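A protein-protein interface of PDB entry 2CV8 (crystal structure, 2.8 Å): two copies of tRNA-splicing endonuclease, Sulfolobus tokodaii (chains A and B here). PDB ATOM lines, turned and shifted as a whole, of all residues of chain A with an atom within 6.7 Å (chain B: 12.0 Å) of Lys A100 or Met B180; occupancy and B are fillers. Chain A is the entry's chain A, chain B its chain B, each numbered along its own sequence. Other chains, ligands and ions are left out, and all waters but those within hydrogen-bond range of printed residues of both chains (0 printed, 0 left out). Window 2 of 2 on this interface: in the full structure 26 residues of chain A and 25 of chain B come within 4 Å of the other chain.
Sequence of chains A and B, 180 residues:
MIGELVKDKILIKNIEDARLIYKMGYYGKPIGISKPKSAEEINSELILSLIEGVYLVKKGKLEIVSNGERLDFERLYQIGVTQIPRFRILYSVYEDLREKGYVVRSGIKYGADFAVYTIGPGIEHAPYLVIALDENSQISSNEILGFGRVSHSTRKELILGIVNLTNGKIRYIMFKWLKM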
ATOM      1  N   TYR A  55      13.695 -11.716  34.941  1.00  0.00           N
ATOM      2  CA  TYR A  55      12.557 -11.958  34.061  1.00  0.00           C
ATOM      3  C   TYR A  55      11.689 -10.708  33.971  1.00  0.00           C
ATOM      4  O   TYR A  55      11.439 -10.196  32.881  1.00  0.00           O
ATOM      5  CB  TYR A  55      11.698 -13.123  34.570  1.00  0.00           C
ATOM      6  CG  TYR A  55      10.537 -13.440  33.649  1.00  0.00           C
ATOM      7  CD1 TYR A  55      10.760 -13.789  32.312  1.00  0.00           C
ATOM      8  CD2 TYR A  55       9.216 -13.334  34.090  1.00  0.00           C
ATOM      9  CE1 TYR A  55       9.703 -14.016  31.441  1.00  0.00           C
ATOM     10  CE2 TYR A  55       8.145 -13.557  33.217  1.00  0.00           C
ATOM     11  CZ  TYR A  55       8.402 -13.895  31.897  1.00  0.00           C
ATOM     12  OH  TYR A  55       7.359 -14.104  31.032  1.00  0.00           O
ATOM     13  N   TYR A  94      12.968 -21.160  33.657  1.00  0.00           N
ATOM     14  CA  TYR A  94      12.046 -20.241  34.314  1.00  0.00           C
ATOM     15  C   TYR A  94      11.307 -19.421  33.272  1.00  0.00           C
ATOM     16  O   TYR A  94      10.073 -19.400  33.227  1.00  0.00           O
ATOM     17  CB  TYR A  94      12.770 -19.277  35.250  1.00  0.00           C
ATOM     18  CG  TYR A  94      11.793 -18.360  35.960  1.00  0.00           C
ATOM     19  CD1 TYR A  94      11.164 -18.757  37.134  1.00  0.00           C
ATOM     20  CD2 TYR A  94      11.432 -17.137  35.411  1.00  0.00           C
ATOM     21  CE1 TYR A  94      10.196 -17.959  37.740  1.00  0.00           C
ATOM     22  CE2 TYR A  94      10.461 -16.332  36.009  1.00  0.00           C
ATOM     23  CZ  TYR A  94       9.849 -16.750  37.170  1.00  0.00           C
ATOM     24  OH  TYR A  94       8.883 -15.968  37.753  1.00  0.00           O
ATOM     25  N   GLU A  95      12.089 -18.746  32.441  1.00  0.00           N
ATOM     26  CA  GLU A  95      11.583 -17.899  31.378  1.00  0.00           C
ATOM     27  C   GLU A  95      10.676 -18.635  30.389  1.00  0.00           C
ATOM     28  O   GLU A  95       9.559 -18.201  30.116  1.00  0.00           O
ATOM     29  CB  GLU A  95      12.756 -17.293  30.626  1.00  0.00           C
ATOM     30  CG  GLU A  95      12.350 -16.366  29.508  1.00  0.00           C
ATOM     31  CD  GLU A  95      13.531 -15.954  28.666  1.00  0.00           C
ATOM     32  OE1 GLU A  95      14.129 -16.837  28.017  1.00  0.00           O
ATOM     33  OE2 GLU A  95      13.867 -14.752  28.658  1.00  0.00           O
ATOM     34  N   ASP A  96      11.172 -19.742  29.850  1.00  0.00           N
ATOM     35  CA  ASP A  96      10.422 -20.530  28.884  1.00  0.00           C
ATOM     36  C   ASP A  96       9.073 -20.928  29.469  1.00  0.00           C
ATOM     37  O   ASP A  96       8.038 -20.756  28.827  1.00  0.00           O
ATOM     38  CB  ASP A  96      11.233 -21.780  28.489  1.00  0.00           C
ATOM     39  CG  ASP A  96      10.534 -22.640  27.435  1.00  0.00           C
ATOM     40  OD1 ASP A  96       9.940 -23.681  27.788  1.00  0.00           O
ATOM     41  OD2 ASP A  96      10.576 -22.274  26.246  1.00  0.00           O
ATOM     42  N   LEU A  97       9.083 -21.446  30.692  1.00  0.00           N
ATOM     43  CA  LEU A  97       7.848 -21.871  31.313  1.00  0.00           C
ATOM     44  C   LEU A  97       6.951 -20.684  31.618  1.00  0.00           C
ATOM     45  O   LEU A  97       5.722 -20.728  31.441  1.00  0.00           O
ATOM     46  CB  LEU A  97       8.149 -22.638  32.590  1.00  0.00           C
ATOM     47  CG  LEU A  97       8.672 -24.049  32.368  1.00  0.00           C
ATOM     48  CD1 LEU A  97       8.738 -24.787  33.700  1.00  0.00           C
ATOM     49  CD2 LEU A  97       7.749 -24.764  31.396  1.00  0.00           C
ATOM     50  N   ARG A  98       7.567 -19.613  32.082  1.00  0.00           N
ATOM     51  CA  ARG A  98       6.810 -18.421  32.409  1.00  0.00           C
ATOM     52  C   ARG A  98       6.206 -17.839  31.123  1.00  0.00           C
ATOM     53  O   ARG A  98       5.033 -17.461  31.074  1.00  0.00           O
ATOM     54  CB  ARG A  98       7.733 -17.403  33.073  1.00  0.00           C
ATOM     55  CG  ARG A  98       7.021 -16.492  34.026  1.00  0.00           C
ATOM     56  CD  ARG A  98       6.717 -17.160  35.345  1.00  0.00           C
ATOM     57  NE  ARG A  98       5.576 -16.515  35.987  1.00  0.00           N
ATOM     58  CZ  ARG A  98       5.336 -16.538  37.290  1.00  0.00           C
ATOM     59  NH1 ARG A  98       6.158 -17.167  38.111  1.00  0.00           N
ATOM     60  NH2 ARG A  98       4.266 -15.939  37.767  1.00  0.00           N
ATOM     61  N   GLU A  99       7.021 -17.794  30.077  1.00  0.00           N
ATOM     62  CA  GLU A  99       6.595 -17.258  28.796  1.00  0.00           C
ATOM     63  C   GLU A  99       5.447 -18.075  28.226  1.00  0.00           C
ATOM     64  O   GLU A  99       4.649 -17.563  27.442  1.00  0.00           O
ATOM     65  CB  GLU A  99       7.774 -17.255  27.818  1.00  0.00           C
ATOM     66  CG  GLU A  99       7.667 -16.209  26.725  1.00  0.00           C
ATOM     67  CD  GLU A  99       7.694 -14.791  27.266  1.00  0.00           C
ATOM     68  OE1 GLU A  99       7.445 -13.856  26.481  1.00  0.00           O
ATOM     69  OE2 GLU A  99       7.964 -14.602  28.468  1.00  0.00           O
ATOM     70  N   LYS A 100       5.372 -19.343  28.620  1.00  0.00           N
ATOM     71  CA  LYS A 100       4.318 -20.232  28.142  1.00  0.00           C
ATOM     72  C   LYS A 100       3.059 -20.099  28.971  1.00  0.00           C
ATOM     73  O   LYS A 100       2.079 -20.806  28.745  1.00  0.00           O
ATOM     74  CB  LYS A 100       4.793 -21.688  28.134  1.00  0.00           C
ATOM     75  CG  LYS A 100       5.672 -22.015  26.939  1.00  0.00           C
ATOM     76  CD  LYS A 100       6.165 -23.455  26.963  1.00  0.00           C
ATOM     77  CE  LYS A 100       7.182 -23.682  25.852  1.00  0.00           C
ATOM     78  NZ  LYS A 100       7.852 -25.010  25.943  1.00  0.00           N
ATOM     79  N   GLY A 101       3.092 -19.199  29.945  1.00  0.00           N
ATOM     80  CA  GLY A 101       1.911 -18.975  30.762  1.00  0.00           C
ATOM     81  C   GLY A 101       1.778 -19.712  32.082  1.00  0.00           C
ATOM     82  O   GLY A 101       0.788 -19.533  32.792  1.00  0.00           O
ATOM     83  N   TYR A 102       2.743 -20.555  32.421  1.00  0.00           N
ATOM     84  CA  TYR A 102       2.658 -21.259  33.688  1.00  0.00           C
ATOM     85  C   TYR A 102       3.064 -20.291  34.798  1.00  0.00           C
ATOM     86  O   TYR A 102       3.726 -19.288  34.541  1.00  0.00           O
ATOM     87  CB  TYR A 102       3.613 -22.460  33.725  1.00  0.00           C
ATOM     88  CG  TYR A 102       3.358 -23.546  32.706  1.00  0.00           C
ATOM     89  CD1 TYR A 102       3.767 -23.399  31.387  1.00  0.00           C
ATOM     90  CD2 TYR A 102       2.750 -24.745  33.074  1.00  0.00           C
ATOM     91  CE1 TYR A 102       3.584 -24.429  30.452  1.00  0.00           C
ATOM     92  CE2 TYR A 102       2.563 -25.775  32.151  1.00  0.00           C
ATOM     93  CZ  TYR A 102       2.983 -25.616  30.843  1.00  0.00           C
ATOM     94  OH  TYR A 102       2.811 -26.642  29.929  1.00  0.00           O
ATOM     95  N   VAL A 116       5.839 -25.758  39.078  1.00  0.00           N
ATOM     96  CA  VAL A 116       5.055 -25.138  38.032  1.00  0.00           C
ATOM     97  C   VAL A 116       3.555 -25.388  38.199  1.00  0.00           C
ATOM     98  O   VAL A 116       3.123 -26.517  38.449  1.00  0.00           O
ATOM     99  CB  VAL A 116       5.518 -25.651  36.659  1.00  0.00           C
ATOM    100  CG1 VAL A 116       4.870 -24.851  35.548  1.00  0.00           C
ATOM    101  CG2 VAL A 116       7.018 -25.547  36.568  1.00  0.00           C
ATOM    102  N   TYR A 128       3.626 -29.285  39.209  1.00  0.00           N
ATOM    103  CA  TYR A 128       4.544 -30.162  38.505  1.00  0.00           C
ATOM    104  C   TYR A 128       5.914 -29.746  38.994  1.00  0.00           C
ATOM    105  O   TYR A 128       6.199 -28.557  39.093  1.00  0.00           O
ATOM    106  CB  TYR A 128       4.442 -29.977  36.984  1.00  0.00           C
ATOM    107  CG  TYR A 128       3.126 -30.444  36.435  1.00  0.00           C
ATOM    108  CD1 TYR A 128       2.088 -29.544  36.202  1.00  0.00           C
ATOM    109  CD2 TYR A 128       2.879 -31.803  36.243  1.00  0.00           C
ATOM    110  CE1 TYR A 128       0.826 -29.989  35.795  1.00  0.00           C
ATOM    111  CE2 TYR A 128       1.625 -32.260  35.839  1.00  0.00           C
ATOM    112  CZ  TYR A 128       0.603 -31.350  35.620  1.00  0.00           C
ATOM    113  OH  TYR A 128      -0.640 -31.806  35.246  1.00  0.00           O
ATOM    114  N   VAL A 130       9.871 -29.491  38.464  1.00  0.00           N
ATOM    115  CA  VAL A 130      10.843 -29.495  37.383  1.00  0.00           C
ATOM    116  C   VAL A 130      12.267 -29.279  37.888  1.00  0.00           C
ATOM    117  O   VAL A 130      12.514 -28.505  38.820  1.00  0.00           O
ATOM    118  CB  VAL A 130      10.539 -28.386  36.328  1.00  0.00           C
ATOM    119  CG1 VAL A 130      11.523 -28.497  35.184  1.00  0.00           C
ATOM    120  CG2 VAL A 130       9.106 -28.482  35.825  1.00  0.00           C
ATOM    121  N   ILE A 159       9.535 -33.569  36.270  1.00  0.00           N
ATOM    122  CA  ILE A 159       9.857 -33.177  34.892  1.00  0.00           C
ATOM    123  C   ILE A 159      11.293 -32.658  34.757  1.00  0.00           C
ATOM    124  O   ILE A 159      11.740 -31.793  35.519  1.00  0.00           O
ATOM    125  CB  ILE A 159       8.887 -32.088  34.336  1.00  0.00           C
ATOM    126  CG1 ILE A 159       7.471 -32.649  34.227  1.00  0.00           C
ATOM    127  CG2 ILE A 159       9.348 -31.623  32.952  1.00  0.00           C
ATOM    128  CD1 ILE A 159       6.477 -31.686  33.604  1.00  0.00           C
ATOM    129  N   ILE A 170      15.040 -25.846  24.662  1.00  0.00           N
ATOM    130  CA  ILE A 170      14.766 -26.707  25.819  1.00  0.00           C
ATOM    131  C   ILE A 170      13.871 -27.923  25.511  1.00  0.00           C
ATOM    132  O   ILE A 170      12.827 -27.808  24.859  1.00  0.00           O
ATOM    133  CB  ILE A 170      14.077 -25.895  26.935  1.00  0.00           C
ATOM    134  CG1 ILE A 170      14.878 -24.632  27.227  1.00  0.00           C
ATOM    135  CG2 ILE A 170      13.903 -26.756  28.179  1.00  0.00           C
ATOM    136  CD1 ILE A 170      14.242 -23.733  28.238  1.00  0.00           C
ATOM    137  N   TYR A 172      11.710 -30.883  27.287  1.00  0.00           N
ATOM    138  CA  TYR A 172      11.135 -31.302  28.548  1.00  0.00           C
ATOM    139  C   TYR A 172      10.754 -32.765  28.480  1.00  0.00           C
ATOM    140  O   TYR A 172      10.054 -33.195  27.565  1.00  0.00           O
ATOM    141  CB  TYR A 172       9.904 -30.441  28.889  1.00  0.00           C
ATOM    142  CG  TYR A 172      10.252 -29.026  29.302  1.00  0.00           C
ATOM    143  CD1 TYR A 172      10.087 -27.964  28.426  1.00  0.00           C
ATOM    144  CD2 TYR A 172      10.773 -28.760  30.570  1.00  0.00           C
ATOM    145  CE1 TYR A 172      10.428 -26.669  28.795  1.00  0.00           C
ATOM    146  CE2 TYR A 172      11.122 -27.466  30.949  1.00  0.00           C
ATOM    147  CZ  TYR A 172      10.947 -26.424  30.053  1.00  0.00           C
ATOM    148  OH  TYR A 172      11.309 -25.144  30.406  1.00  0.00           O
ATOM    149  N   HIS B 152       9.085 -40.972  21.118  1.00  0.00           N
ATOM    150  CA  HIS B 152       8.137 -40.417  20.160  1.00  0.00           C
ATOM    151  C   HIS B 152       8.539 -40.648  18.703  1.00  0.00           C
ATOM    152  O   HIS B 152       8.280 -39.811  17.838  1.00  0.00           O
ATOM    153  CB  HIS B 152       7.922 -38.921  20.423  1.00  0.00           C
ATOM    154  CG  HIS B 152       6.882 -38.636  21.466  1.00  0.00           C
ATOM    155  ND1 HIS B 152       6.482 -37.358  21.792  1.00  0.00           N
ATOM    156  CD2 HIS B 152       6.147 -39.468  22.244  1.00  0.00           C
ATOM    157  CE1 HIS B 152       5.546 -37.414  22.722  1.00  0.00           C
ATOM    158  NE2 HIS B 152       5.324 -38.682  23.015  1.00  0.00           N
ATOM    159  N   ARG B 155       6.106 -43.639  18.515  1.00  0.00           N
ATOM    160  CA  ARG B 155       5.136 -43.167  19.491  1.00  0.00           C
ATOM    161  C   ARG B 155       4.505 -44.294  20.305  1.00  0.00           C
ATOM    162  O   ARG B 155       3.284 -44.454  20.337  1.00  0.00           O
ATOM    163  CB  ARG B 155       4.051 -42.335  18.800  1.00  0.00           C
ATOM    164  CG  ARG B 155       3.651 -41.093  19.592  1.00  0.00           C
ATOM    165  CD  ARG B 155       3.058 -41.463  20.947  1.00  0.00           C
ATOM    166  NE  ARG B 155       3.022 -40.330  21.869  1.00  0.00           N
ATOM    167  CZ  ARG B 155       2.426 -40.351  23.058  1.00  0.00           C
ATOM    168  NH1 ARG B 155       1.807 -41.449  23.476  1.00  0.00           N
ATOM    169  NH2 ARG B 155       2.455 -39.277  23.835  1.00  0.00           N
ATOM    170  N   LYS B 176       7.979 -39.651  28.864  1.00  0.00           N
ATOM    171  CA  LYS B 176       7.512 -39.201  27.572  1.00  0.00           C
ATOM    172  C   LYS B 176       8.165 -37.887  27.199  1.00  0.00           C
ATOM    173  O   LYS B 176       8.562 -37.123  28.065  1.00  0.00           O
ATOM    174  CB  LYS B 176       5.997 -39.005  27.603  1.00  0.00           C
ATOM    175  CG  LYS B 176       5.226 -40.226  28.052  1.00  0.00           C
ATOM    176  CD  LYS B 176       3.740 -40.007  27.907  1.00  0.00           C
ATOM    177  CE  LYS B 176       2.964 -41.266  28.230  1.00  0.00           C
ATOM    178  NZ  LYS B 176       1.509 -41.085  27.966  1.00  0.00           N
ATOM    179  N   TRP B 177       8.280 -37.643  25.899  1.00  0.00           N
ATOM    180  CA  TRP B 177       8.836 -36.404  25.389  1.00  0.00           C
ATOM    181  C   TRP B 177       7.652 -35.431  25.462  1.00  0.00           C
ATOM    182  O   TRP B 177       6.652 -35.605  24.764  1.00  0.00           O
ATOM    183  CB  TRP B 177       9.290 -36.604  23.939  1.00  0.00           C
ATOM    184  CG  TRP B 177       9.972 -35.417  23.320  1.00  0.00           C
ATOM    185  CD1 TRP B 177      11.211 -34.930  23.623  1.00  0.00           C
ATOM    186  CD2 TRP B 177       9.452 -34.572  22.280  1.00  0.00           C
ATOM    187  NE1 TRP B 177      11.498 -33.837  22.838  1.00  0.00           N
ATOM    188  CE2 TRP B 177      10.435 -33.594  22.006  1.00  0.00           C
ATOM    189  CE3 TRP B 177       8.249 -34.545  21.556  1.00  0.00           C
ATOM    190  CZ2 TRP B 177      10.255 -32.599  21.036  1.00  0.00           C
ATOM    191  CZ3 TRP B 177       8.071 -33.555  20.592  1.00  0.00           C
ATOM    192  CH2 TRP B 177       9.071 -32.596  20.342  1.00  0.00           C
ATOM    193  N   LEU B 178       7.753 -34.427  26.327  1.00  0.00           N
ATOM    194  CA  LEU B 178       6.676 -33.451  26.494  1.00  0.00           C
ATOM    195  C   LEU B 178       6.763 -32.246  25.574  1.00  0.00           C
ATOM    196  O   LEU B 178       7.831 -31.904  25.077  1.00  0.00           O
ATOM    197  CB  LEU B 178       6.630 -32.945  27.940  1.00  0.00           C
ATOM    198  CG  LEU B 178       6.010 -33.825  29.029  1.00  0.00           C
ATOM    199  CD1 LEU B 178       6.190 -33.165  30.383  1.00  0.00           C
ATOM    200  CD2 LEU B 178       4.536 -34.039  28.730  1.00  0.00           C
ATOM    201  N   LYS B 179       5.623 -31.594  25.375  1.00  0.00           N
ATOM    202  CA  LYS B 179       5.544 -30.406  24.542  1.00  0.00           C
ATOM    203  C   LYS B 179       4.912 -29.301  25.383  1.00  0.00           C
ATOM    204  O   LYS B 179       3.786 -28.876  25.119  1.00  0.00           O
ATOM    205  CB  LYS B 179       4.687 -30.689  23.308  1.00  0.00           C
ATOM    206  CG  LYS B 179       5.152 -31.900  22.515  1.00  0.00           C
ATOM    207  CD  LYS B 179       4.262 -32.157  21.309  1.00  0.00           C
ATOM    208  CE  LYS B 179       4.703 -33.408  20.564  1.00  0.00           C
ATOM    209  NZ  LYS B 179       3.842 -33.688  19.385  1.00  0.00           N
ATOM    210  N   MET B 180       5.643 -28.851  26.400  1.00  0.00           N
ATOM    211  CA  MET B 180       5.171 -27.802  27.302  1.00  0.00           C
ATOM    212  C   MET B 180       4.525 -26.617  26.587  1.00  0.00           C
ATOM    213  O   MET B 180       3.350 -26.325  26.892  1.00  0.00           O
ATOM    214  OXT MET B 180       5.204 -25.992  25.744  1.00  0.00           O
ATOM    215  CB  MET B 180       6.325 -27.290  28.163  1.00  0.00           C
ATOM    216  CG  MET B 180       6.928 -28.335  29.064  1.00  0.00           C
ATOM    217  SD  MET B 180       5.763 -28.959  30.440  1.00  0.00           S
ATOM    218  CE  MET B 180       6.454 -28.002  31.948  1.00  0.00           C
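The chain-end carboxylate (OXT) of Met B180 lies within salt-bridge range of the side-chain amino group (NZ) of Lys A100, at 2.8 Å. O of Tyr A172 is in hydrogen-bond range of N of Leu B178, 2.9 Å away. O of Met B180 lies within hydrogen-bond range of OH of Tyr A102 (3.1 Å).
OD1 of Asp A96 sits close to OH of Tyr A172, 3.3 Å away. The side-chain carboxylate of Asp A96 is in salt-bridge range of the side-chain amino group of Lys A100, 3.1 Å away. The backbone carbonyl oxygen (O) of Leu A97 is in hydrogen-bond range of the backbone NH (N) of Tyr A102, at 3.1 Å. A ring nitrogen (ND1) of His B152 sits close to the backbone carbonyl oxygen (O) of Trp B177 (3.5 Å).
Among the printed residues, pairs that only touch across the chains: Leu A97 with Met B180 (3.5 Å), Ile A159 with Leu B178 (3.6 Å), Tyr A172 with Trp B177 (3.9 Å) and Tyr A172 with Met B180 (3.2 Å).
Lys A100 touches one residue of chain B. Met B180 touches just these residues of chain A: Leu A97, Lys A100, Tyr A102 and Tyr A172. No residue of chain B comes within 4 Å of Asp A96. Leu A97 touches just one residue of chain B: Met B180. No residue of chain B comes within 4 Å of Glu A99. No residue of chain B comes within 4 Å of Val A116. No residue of chain B comes within 4 Å of Ile A170. Printed residues of chain B within 4 Å of Tyr A172: Trp B177 (3.9 Å), Leu B178 (2.9 Å) and Met B180 (3.2 Å). Of the printed residues of chain A, Trp B177 touches Tyr A172. Of the printed residues of chain A, Leu B178 touches Ile A159 and Tyr A172. Tyr A128 touches none of the printed residues of chain B. The nearest residue of chain B that does not touch Lys A100 is Lys B179 (5.2 Å).
Of the 7 printed residues of chain B, 3 touch a printed residue of chain A. Hydrophobic or aromatic side chains of chain A that line the printed part of chain B: Leu A97, Tyr A102, Ile A159 and Tyr A172. Among the printed residues, 7 pairs touch across the chains. Among the printed residues, no Asp or Glu carboxylate lies within 4 Å of a Lys or Arg side-chain nitrogen of the other chain.
No position is printed for both chains. Of the 7 pairs that touch across the chains among the printed residues, none has its exchanged pair printed and touching as well.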
